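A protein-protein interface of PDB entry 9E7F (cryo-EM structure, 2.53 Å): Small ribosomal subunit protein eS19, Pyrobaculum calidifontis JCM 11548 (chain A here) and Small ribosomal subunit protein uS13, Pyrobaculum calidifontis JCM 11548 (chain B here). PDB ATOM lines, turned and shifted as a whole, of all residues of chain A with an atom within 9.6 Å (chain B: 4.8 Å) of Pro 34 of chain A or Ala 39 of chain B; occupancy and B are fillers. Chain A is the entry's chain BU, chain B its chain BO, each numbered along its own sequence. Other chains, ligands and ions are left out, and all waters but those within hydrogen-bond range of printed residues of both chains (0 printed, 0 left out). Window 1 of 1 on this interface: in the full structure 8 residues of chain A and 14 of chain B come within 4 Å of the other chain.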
ATOM      1  N   PRO A  29     -12.291 -15.224   0.225  1.00  0.00           N
ATOM      2  CA  PRO A  29     -13.126 -14.033   0.387  1.00  0.00           C
ATOM      3  C   PRO A  29     -14.584 -14.417   0.535  1.00  0.00           C
ATOM      4  O   PRO A  29     -15.104 -15.229  -0.243  1.00  0.00           O
ATOM      5  CB  PRO A  29     -12.894 -13.242  -0.907  1.00  0.00           C
ATOM      6  CG  PRO A  29     -11.873 -13.955  -1.673  1.00  0.00           C
ATOM      7  CD  PRO A  29     -11.400 -15.150  -0.940  1.00  0.00           C
ATOM      8  N   PRO A  30     -15.275 -13.850   1.512  1.00  0.00           N
ATOM      9  CA  PRO A  30     -16.650 -14.258   1.807  1.00  0.00           C
ATOM     10  C   PRO A  30     -17.637 -13.648   0.818  1.00  0.00           C
ATOM     11  O   PRO A  30     -17.268 -13.008  -0.164  1.00  0.00           O
ATOM     12  CB  PRO A  30     -16.881 -13.737   3.225  1.00  0.00           C
ATOM     13  CG  PRO A  30     -15.761 -12.818   3.528  1.00  0.00           C
ATOM     14  CD  PRO A  30     -14.804 -12.780   2.400  1.00  0.00           C
ATOM     15  N   VAL A  31     -18.922 -13.871   1.098  1.00  0.00           N
ATOM     16  CA  VAL A  31     -19.968 -13.512   0.150  1.00  0.00           C
ATOM     17  C   VAL A  31     -20.236 -12.013   0.146  1.00  0.00           C
ATOM     18  O   VAL A  31     -20.752 -11.474  -0.839  1.00  0.00           O
ATOM     19  CB  VAL A  31     -21.248 -14.304   0.462  1.00  0.00           C
ATOM     20  CG1 VAL A  31     -21.890 -13.781   1.732  1.00  0.00           C
ATOM     21  CG2 VAL A  31     -22.208 -14.214  -0.696  1.00  0.00           C
ATOM     22  N   TRP A  32     -19.923 -11.318   1.233  1.00  0.00           N
ATOM     23  CA  TRP A  32     -20.137  -9.882   1.303  1.00  0.00           C
ATOM     24  C   TRP A  32     -18.910  -9.087   0.896  1.00  0.00           C
ATOM     25  O   TRP A  32     -18.912  -7.862   1.036  1.00  0.00           O
ATOM     26  CB  TRP A  32     -20.572  -9.473   2.710  1.00  0.00           C
ATOM     27  CG  TRP A  32     -19.797 -10.104   3.819  1.00  0.00           C
ATOM     28  CD1 TRP A  32     -20.133 -11.226   4.510  1.00  0.00           C
ATOM     29  CD2 TRP A  32     -18.571  -9.636   4.386  1.00  0.00           C
ATOM     30  NE1 TRP A  32     -19.190 -11.494   5.468  1.00  0.00           N
ATOM     31  CE2 TRP A  32     -18.219 -10.532   5.412  1.00  0.00           C
ATOM     32  CE3 TRP A  32     -17.734  -8.551   4.124  1.00  0.00           C
ATOM     33  CZ2 TRP A  32     -17.067 -10.375   6.173  1.00  0.00           C
ATOM     34  CZ3 TRP A  32     -16.592  -8.396   4.881  1.00  0.00           C
ATOM     35  CH2 TRP A  32     -16.268  -9.305   5.894  1.00  0.00           C
ATOM     36  N   ALA A  33     -17.870  -9.759   0.412  1.00  0.00           N
ATOM     37  CA  ALA A  33     -16.647  -9.076   0.004  1.00  0.00           C
ATOM     38  C   ALA A  33     -16.834  -8.016  -1.077  1.00  0.00           C
ATOM     39  O   ALA A  33     -16.306  -6.906  -0.898  1.00  0.00           O
ATOM     40  CB  ALA A  33     -15.616 -10.112  -0.450  1.00  0.00           C
ATOM     41  N   PRO A  34     -17.530  -8.258  -2.195  1.00  0.00           N
ATOM     42  CA  PRO A  34     -17.626  -7.205  -3.220  1.00  0.00           C
ATOM     43  C   PRO A  34     -18.474  -6.005  -2.829  1.00  0.00           C
ATOM     44  O   PRO A  34     -18.471  -5.014  -3.565  1.00  0.00           O
ATOM     45  CB  PRO A  34     -18.238  -7.923  -4.432  1.00  0.00           C
ATOM     46  CG  PRO A  34     -18.446  -9.308  -4.060  1.00  0.00           C
ATOM     47  CD  PRO A  34     -18.100  -9.539  -2.649  1.00  0.00           C
ATOM     48  N   PHE A  35     -19.192  -6.036  -1.710  1.00  0.00           N
ATOM     49  CA  PHE A  35     -20.112  -4.963  -1.359  1.00  0.00           C
ATOM     50  C   PHE A  35     -19.612  -4.072  -0.233  1.00  0.00           C
ATOM     51  O   PHE A  35     -20.388  -3.263   0.282  1.00  0.00           O
ATOM     52  CB  PHE A  35     -21.475  -5.541  -0.978  1.00  0.00           C
ATOM     53  CG  PHE A  35     -22.036  -6.481  -1.989  1.00  0.00           C
ATOM     54  CD1 PHE A  35     -22.610  -6.005  -3.144  1.00  0.00           C
ATOM     55  CD2 PHE A  35     -21.989  -7.841  -1.785  1.00  0.00           C
ATOM     56  CE1 PHE A  35     -23.126  -6.866  -4.074  1.00  0.00           C
ATOM     57  CE2 PHE A  35     -22.502  -8.705  -2.713  1.00  0.00           C
ATOM     58  CZ  PHE A  35     -23.070  -8.217  -3.859  1.00  0.00           C
ATOM     59  N   VAL A  36     -18.349  -4.184   0.171  1.00  0.00           N
ATOM     60  CA  VAL A  36     -17.881  -3.467   1.348  1.00  0.00           C
ATOM     61  C   VAL A  36     -16.565  -2.762   1.060  1.00  0.00           C
ATOM     62  O   VAL A  36     -15.814  -3.125   0.154  1.00  0.00           O
ATOM     63  CB  VAL A  36     -17.719  -4.395   2.571  1.00  0.00           C
ATOM     64  CG1 VAL A  36     -19.019  -5.104   2.874  1.00  0.00           C
ATOM     65  CG2 VAL A  36     -16.608  -5.389   2.337  1.00  0.00           C
ATOM     66  N   LYS A  37     -16.306  -1.732   1.855  1.00  0.00           N
ATOM     67  CA  LYS A  37     -15.016  -1.078   1.962  1.00  0.00           C
ATOM     68  C   LYS A  37     -14.342  -1.530   3.249  1.00  0.00           C
ATOM     69  O   LYS A  37     -14.978  -2.090   4.144  1.00  0.00           O
ATOM     70  CB  LYS A  37     -15.180   0.442   1.941  1.00  0.00           C
ATOM     71  CG  LYS A  37     -16.209   0.921   0.948  1.00  0.00           C
ATOM     72  CD  LYS A  37     -16.491   2.397   1.092  1.00  0.00           C
ATOM     73  CE  LYS A  37     -17.354   2.884  -0.054  1.00  0.00           C
ATOM     74  NZ  LYS A  37     -17.823   4.279   0.135  1.00  0.00           N
ATOM     75  N   THR A  38     -13.044  -1.279   3.350  1.00  0.00           N
ATOM     76  CA  THR A  38     -12.279  -1.816   4.472  1.00  0.00           C
ATOM     77  C   THR A  38     -12.275  -0.876   5.671  1.00  0.00           C
ATOM     78  O   THR A  38     -11.229  -0.597   6.248  1.00  0.00           O
ATOM     79  CB  THR A  38     -10.857  -2.117   4.021  1.00  0.00           C
ATOM     80  OG1 THR A  38     -10.189  -0.891   3.709  1.00  0.00           O
ATOM     81  CG2 THR A  38     -10.871  -3.000   2.795  1.00  0.00           C
ATOM     82  N   ARG A  44     -13.878   4.738  -1.073  1.00  0.00           N
ATOM     83  CA  ARG A  44     -14.096   3.808  -2.167  1.00  0.00           C
ATOM     84  C   ARG A  44     -13.671   2.410  -1.762  1.00  0.00           C
ATOM     85  O   ARG A  44     -12.876   2.239  -0.833  1.00  0.00           O
ATOM     86  CB  ARG A  44     -13.318   4.246  -3.415  1.00  0.00           C
ATOM     87  CG  ARG A  44     -13.836   5.514  -4.014  1.00  0.00           C
ATOM     88  CD  ARG A  44     -13.171   5.819  -5.328  1.00  0.00           C
ATOM     89  NE  ARG A  44     -13.399   7.206  -5.707  1.00  0.00           N
ATOM     90  CZ  ARG A  44     -12.449   8.037  -6.102  1.00  0.00           C
ATOM     91  NH1 ARG A  44     -11.198   7.640  -6.241  1.00  0.00           N
ATOM     92  NH2 ARG A  44     -12.763   9.301  -6.355  1.00  0.00           N
ATOM     93  N   PRO A  45     -14.183   1.389  -2.437  1.00  0.00           N
ATOM     94  CA  PRO A  45     -13.762   0.031  -2.139  1.00  0.00           C
ATOM     95  C   PRO A  45     -12.355  -0.209  -2.646  1.00  0.00           C
ATOM     96  O   PRO A  45     -11.859   0.551  -3.490  1.00  0.00           O
ATOM     97  CB  PRO A  45     -14.781  -0.833  -2.889  1.00  0.00           C
ATOM     98  CG  PRO A  45     -15.338   0.034  -3.941  1.00  0.00           C
ATOM     99  CD  PRO A  45     -15.034   1.457  -3.636  1.00  0.00           C
ATOM    100  N   PRO A  46     -11.674  -1.233  -2.140  1.00  0.00           N
ATOM    101  CA  PRO A  46     -10.323  -1.526  -2.624  1.00  0.00           C
ATOM    102  C   PRO A  46     -10.349  -1.943  -4.083  1.00  0.00           C
ATOM    103  O   PRO A  46     -11.270  -2.623  -4.537  1.00  0.00           O
ATOM    104  CB  PRO A  46      -9.848  -2.662  -1.716  1.00  0.00           C
ATOM    105  CG  PRO A  46     -10.924  -2.901  -0.733  1.00  0.00           C
ATOM    106  CD  PRO A  46     -12.155  -2.213  -1.158  1.00  0.00           C
ATOM    107  N   SER A  48      -7.725  -3.555  -6.098  1.00  0.00           N
ATOM    108  CA  SER A  48      -7.147  -4.841  -6.455  1.00  0.00           C
ATOM    109  C   SER A  48      -8.046  -5.985  -6.020  1.00  0.00           C
ATOM    110  O   SER A  48      -8.418  -6.088  -4.848  1.00  0.00           O
ATOM    111  CB  SER A  48      -5.770  -4.976  -5.810  1.00  0.00           C
ATOM    112  OG  SER A  48      -5.422  -6.336  -5.638  1.00  0.00           O
ATOM    113  N   GLU A  49      -8.382  -6.860  -6.968  1.00  0.00           N
ATOM    114  CA  GLU A  49      -9.275  -7.975  -6.685  1.00  0.00           C
ATOM    115  C   GLU A  49      -8.682  -8.976  -5.708  1.00  0.00           C
ATOM    116  O   GLU A  49      -9.438  -9.734  -5.095  1.00  0.00           O
ATOM    117  CB  GLU A  49      -9.653  -8.685  -7.982  1.00  0.00           C
ATOM    118  CG  GLU A  49     -11.023  -8.303  -8.515  1.00  0.00           C
ATOM    119  CD  GLU A  49     -11.044  -6.925  -9.146  1.00  0.00           C
ATOM    120  OE1 GLU A  49     -10.225  -6.674 -10.053  1.00  0.00           O
ATOM    121  OE2 GLU A  49     -11.883  -6.093  -8.741  1.00  0.00           O
ATOM    122  N   TRP A  51      -7.420  -8.197  -2.902  1.00  0.00           N
ATOM    123  CA  TRP A  51      -7.252  -7.433  -1.672  1.00  0.00           C
ATOM    124  C   TRP A  51      -7.488  -8.285  -0.435  1.00  0.00           C
ATOM    125  O   TRP A  51      -6.930  -7.994   0.627  1.00  0.00           O
ATOM    126  CB  TRP A  51      -8.171  -6.212  -1.679  1.00  0.00           C
ATOM    127  CG  TRP A  51      -9.630  -6.496  -1.516  1.00  0.00           C
ATOM    128  CD1 TRP A  51     -10.536  -6.697  -2.508  1.00  0.00           C
ATOM    129  CD2 TRP A  51     -10.356  -6.578  -0.289  1.00  0.00           C
ATOM    130  NE1 TRP A  51     -11.780  -6.914  -1.976  1.00  0.00           N
ATOM    131  CE2 TRP A  51     -11.693  -6.848  -0.612  1.00  0.00           C
ATOM    132  CE3 TRP A  51     -10.000  -6.460   1.054  1.00  0.00           C
ATOM    133  CZ2 TRP A  51     -12.675  -6.996   0.355  1.00  0.00           C
ATOM    134  CZ3 TRP A  51     -10.975  -6.607   2.009  1.00  0.00           C
ATOM    135  CH2 TRP A  51     -12.297  -6.874   1.658  1.00  0.00           C
ATOM    136  N   TRP A  52      -8.312  -9.326  -0.541  1.00  0.00           N
ATOM    137  CA  TRP A  52      -8.490 -10.224   0.591  1.00  0.00           C
ATOM    138  C   TRP A  52      -7.207 -10.980   0.898  1.00  0.00           C
ATOM    139  O   TRP A  52      -6.820 -11.117   2.063  1.00  0.00           O
ATOM    140  CB  TRP A  52      -9.627 -11.199   0.313  1.00  0.00           C
ATOM    141  CG  TRP A  52     -10.023 -11.990   1.500  1.00  0.00           C
ATOM    142  CD1 TRP A  52      -9.554 -13.211   1.862  1.00  0.00           C
ATOM    143  CD2 TRP A  52     -10.977 -11.617   2.494  1.00  0.00           C
ATOM    144  NE1 TRP A  52     -10.155 -13.624   3.018  1.00  0.00           N
ATOM    145  CE2 TRP A  52     -11.036 -12.661   3.427  1.00  0.00           C
ATOM    146  CE3 TRP A  52     -11.788 -10.497   2.683  1.00  0.00           C
ATOM    147  CZ2 TRP A  52     -11.872 -12.622   4.533  1.00  0.00           C
ATOM    148  CZ3 TRP A  52     -12.614 -10.461   3.778  1.00  0.00           C
ATOM    149  CH2 TRP A  52     -12.652 -11.515   4.691  1.00  0.00           C
ATOM    150  N   ILE A 100     -13.626  -7.798   8.683  1.00  0.00           N
ATOM    151  CA  ILE A 100     -12.611  -8.300   7.765  1.00  0.00           C
ATOM    152  C   ILE A 100     -11.423  -8.850   8.540  1.00  0.00           C
ATOM    153  O   ILE A 100     -10.931  -9.945   8.259  1.00  0.00           O
ATOM    154  CB  ILE A 100     -12.176  -7.194   6.788  1.00  0.00           C
ATOM    155  CG1 ILE A 100     -13.349  -6.741   5.922  1.00  0.00           C
ATOM    156  CG2 ILE A 100     -11.024  -7.667   5.927  1.00  0.00           C
ATOM    157  CD1 ILE A 100     -14.138  -5.588   6.509  1.00  0.00           C
ATOM    158  N   ALA B  35     -19.460   2.825  -5.376  1.00  0.00           N
ATOM    159  CA  ALA B  35     -19.584   1.619  -4.565  1.00  0.00           C
ATOM    160  C   ALA B  35     -20.525   0.622  -5.224  1.00  0.00           C
ATOM    161  O   ALA B  35     -20.231  -0.576  -5.299  1.00  0.00           O
ATOM    162  CB  ALA B  35     -20.068   1.976  -3.162  1.00  0.00           C
ATOM    163  N   THR B  36     -21.659   1.106  -5.725  1.00  0.00           N
ATOM    164  CA  THR B  36     -22.589   0.232  -6.425  1.00  0.00           C
ATOM    165  C   THR B  36     -21.996  -0.276  -7.730  1.00  0.00           C
ATOM    166  O   THR B  36     -22.161  -1.451  -8.074  1.00  0.00           O
ATOM    167  CB  THR B  36     -23.900   0.969  -6.679  1.00  0.00           C
ATOM    168  OG1 THR B  36     -24.692   0.953  -5.488  1.00  0.00           O
ATOM    169  CG2 THR B  36     -24.668   0.301  -7.786  1.00  0.00           C
ATOM    170  N   ALA B  37     -21.303   0.593  -8.470  1.00  0.00           N
ATOM    171  CA  ALA B  37     -20.729   0.195  -9.750  1.00  0.00           C
ATOM    172  C   ALA B  37     -19.628  -0.837  -9.573  1.00  0.00           C
ATOM    173  O   ALA B  37     -19.501  -1.762 -10.380  1.00  0.00           O
ATOM    174  CB  ALA B  37     -20.190   1.416 -10.486  1.00  0.00           C
ATOM    175  N   TYR B  38     -18.811  -0.684  -8.533  1.00  0.00           N
ATOM    176  CA  TYR B  38     -17.774  -1.671  -8.249  1.00  0.00           C
ATOM    177  C   TYR B  38     -18.372  -3.015  -7.857  1.00  0.00           C
ATOM    178  O   TYR B  38     -17.840  -4.065  -8.224  1.00  0.00           O
ATOM    179  CB  TYR B  38     -16.862  -1.164  -7.141  1.00  0.00           C
ATOM    180  CG  TYR B  38     -15.515  -0.696  -7.617  1.00  0.00           C
ATOM    181  CD1 TYR B  38     -14.502  -1.598  -7.874  1.00  0.00           C
ATOM    182  CD2 TYR B  38     -15.255   0.647  -7.794  1.00  0.00           C
ATOM    183  CE1 TYR B  38     -13.272  -1.176  -8.297  1.00  0.00           C
ATOM    184  CE2 TYR B  38     -14.030   1.076  -8.214  1.00  0.00           C
ATOM    185  CZ  TYR B  38     -13.042   0.162  -8.463  1.00  0.00           C
ATOM    186  OH  TYR B  38     -11.813   0.588  -8.887  1.00  0.00           O
ATOM    187  N   ALA B  39     -19.461  -3.004  -7.094  1.00  0.00           N
ATOM    188  CA  ALA B  39     -20.064  -4.264  -6.677  1.00  0.00           C
ATOM    189  C   ALA B  39     -20.686  -4.999  -7.853  1.00  0.00           C
ATOM    190  O   ALA B  39     -20.631  -6.230  -7.917  1.00  0.00           O
ATOM    191  CB  ALA B  39     -21.106  -4.020  -5.588  1.00  0.00           C
ATOM    192  N   ILE B  40     -21.282  -4.264  -8.791  1.00  0.00           N
ATOM    193  CA  ILE B  40     -21.936  -4.897  -9.932  1.00  0.00           C
ATOM    194  C   ILE B  40     -20.909  -5.580 -10.824  1.00  0.00           C
ATOM    195  O   ILE B  40     -21.143  -6.677 -11.341  1.00  0.00           O
ATOM    196  CB  ILE B  40     -22.760  -3.867 -10.717  1.00  0.00           C
ATOM    197  CG1 ILE B  40     -24.074  -3.591  -9.997  1.00  0.00           C
ATOM    198  CG2 ILE B  40     -23.034  -4.374 -12.104  1.00  0.00           C
ATOM    199  CD1 ILE B  40     -24.795  -2.380 -10.502  1.00  0.00           C
ATOM    200  N   CYS B  41     -19.762  -4.935 -11.028  1.00  0.00           N
ATOM    201  CA  CYS B  41     -18.723  -5.524 -11.863  1.00  0.00           C
ATOM    202  C   CYS B  41     -18.140  -6.773 -11.215  1.00  0.00           C
ATOM    203  O   CYS B  41     -17.998  -7.812 -11.866  1.00  0.00           O
ATOM    204  CB  CYS B  41     -17.631  -4.493 -12.138  1.00  0.00           C
ATOM    205  SG  CYS B  41     -18.093  -3.223 -13.329  1.00  0.00           S
ATOM    206  N   ARG B  42     -17.804  -6.690  -9.927  1.00  0.00           N
ATOM    207  CA  ARG B  42     -17.235  -7.841  -9.234  1.00  0.00           C
ATOM    208  C   ARG B  42     -18.243  -8.975  -9.118  1.00  0.00           C
ATOM    209  O   ARG B  42     -17.892 -10.147  -9.293  1.00  0.00           O
ATOM    210  CB  ARG B  42     -16.749  -7.428  -7.847  1.00  0.00           C
ATOM    211  CG  ARG B  42     -15.262  -7.209  -7.755  1.00  0.00           C
ATOM    212  CD  ARG B  42     -14.948  -6.047  -6.847  1.00  0.00           C
ATOM    213  NE  ARG B  42     -13.643  -5.479  -7.142  1.00  0.00           N
ATOM    214  CZ  ARG B  42     -13.052  -4.542  -6.418  1.00  0.00           C
ATOM    215  NH1 ARG B  42     -13.625  -4.039  -5.338  1.00  0.00           N
ATOM    216  NH2 ARG B  42     -11.858  -4.095  -6.789  1.00  0.00           N
ATOM    217  N   LYS B  43     -19.498  -8.639  -8.818  1.00  0.00           N
ATOM    218  CA  LYS B  43     -20.529  -9.653  -8.631  1.00  0.00           C
ATOM    219  C   LYS B  43     -20.806 -10.413  -9.918  1.00  0.00           C
ATOM    220  O   LYS B  43     -21.014 -11.630  -9.897  1.00  0.00           O
ATOM    221  CB  LYS B  43     -21.807  -8.997  -8.124  1.00  0.00           C
ATOM    222  CG  LYS B  43     -22.867  -9.965  -7.691  1.00  0.00           C
ATOM    223  CD  LYS B  43     -22.472 -10.681  -6.427  1.00  0.00           C
ATOM    224  CE  LYS B  43     -23.581 -11.602  -5.993  1.00  0.00           C
ATOM    225  NZ  LYS B  43     -23.466 -12.929  -6.650  1.00  0.00           N
ATOM    226  N   LEU B  44     -20.817  -9.715 -11.045  1.00  0.00           N
ATOM    227  CA  LEU B  44     -21.087 -10.341 -12.329  1.00  0.00           C
ATOM    228  C   LEU B  44     -19.837 -10.897 -12.986  1.00  0.00           C
ATOM    229  O   LEU B  44     -19.913 -11.369 -14.125  1.00  0.00           O
ATOM    230  CB  LEU B  44     -21.756  -9.341 -13.266  1.00  0.00           C
ATOM    231  CG  LEU B  44     -23.117  -8.813 -12.830  1.00  0.00           C
ATOM    232  CD1 LEU B  44     -23.588  -7.754 -13.802  1.00  0.00           C
ATOM    233  CD2 LEU B  44     -24.110  -9.946 -12.743  1.00  0.00           C
ATOM    234  N   PHE B  78     -27.494  -2.393   0.884  1.00  0.00           N
ATOM    235  CA  PHE B  78     -26.701  -1.783  -0.164  1.00  0.00           C
ATOM    236  C   PHE B  78     -27.546  -1.017  -1.167  1.00  0.00           C
ATOM    237  O   PHE B  78     -26.991  -0.442  -2.107  1.00  0.00           O
ATOM    238  CB  PHE B  78     -25.894  -2.871  -0.879  1.00  0.00           C
ATOM    239  CG  PHE B  78     -24.662  -2.376  -1.561  1.00  0.00           C
ATOM    240  CD1 PHE B  78     -23.618  -1.849  -0.837  1.00  0.00           C
ATOM    241  CD2 PHE B  78     -24.542  -2.464  -2.932  1.00  0.00           C
ATOM    242  CE1 PHE B  78     -22.486  -1.401  -1.471  1.00  0.00           C
ATOM    243  CE2 PHE B  78     -23.414  -2.021  -3.566  1.00  0.00           C
ATOM    244  CZ  PHE B  78     -22.385  -1.491  -2.837  1.00  0.00           C
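The guanidinium group of Arg 42 of chain B is in salt-bridge range of the side-chain carboxylate of Glu 49 of chain A.
NH2 of Arg 42 of chain B is in hydrogen-bond range of O of Pro 46 of chain A, at 2.8 Å.
Among the printed residues, merely in contact across the chains: Phe 35 of chain A with Phe 78 of chain B, Pro 34 of chain A with Ala 39 of chain B, Phe 35 of chain A with Ala 39 of chain B, Phe 35 of chain A with Lys 43 of chain B, Pro 45 of chain A with Tyr 38 of chain B and Pro 34 of chain A with Arg 42 of chain B.
Of chain B, only Ala 39 (3.5 Å) and Arg 42 (3.8 Å) come within 4 Å of Pro 34 of chain A.
Of chain A, only Pro 34 and Phe 35 come within 4 Å of Ala 39 of chain B.
No residue of chain A comes within 4 Å of Ile 40 of chain B.
Printed residues of chain A within 4 Å of Tyr 38 of chain B: Pro 45.
Of the printed residues of chain A, Arg 42 of chain B touches Pro 34 (3.8 Å), Pro 46 (2.8 Å) and Glu 49 (2.5 Å).
Printed residues of chain B within 4 Å of Pro 45 of chain A: Tyr 38.
Of the printed residues of chain B, Pro 46 of chain A touches Arg 42 (2.8 Å).
Printed residues of chain B within 4 Å of Glu 49 of chain A: Arg 42 (2.5 Å).
Ser 48 of chain A touches none of the printed residues of chain B.
Thr 36 of chain B touches none of the printed residues of chain A.
The nearest residue of chain B that does not touch Pro 34 of chain A is Lys 43 of chain B (4.6 Å).
The nearest printed residue of chain A that does not touch Tyr 38 of chain B is Pro 46 of chain A (4.5 Å).
Along chain A the printed residues that touch a printed residue of chain B span positions 34 to 49.
Among the printed residues, 8 pairs touch across the chains.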
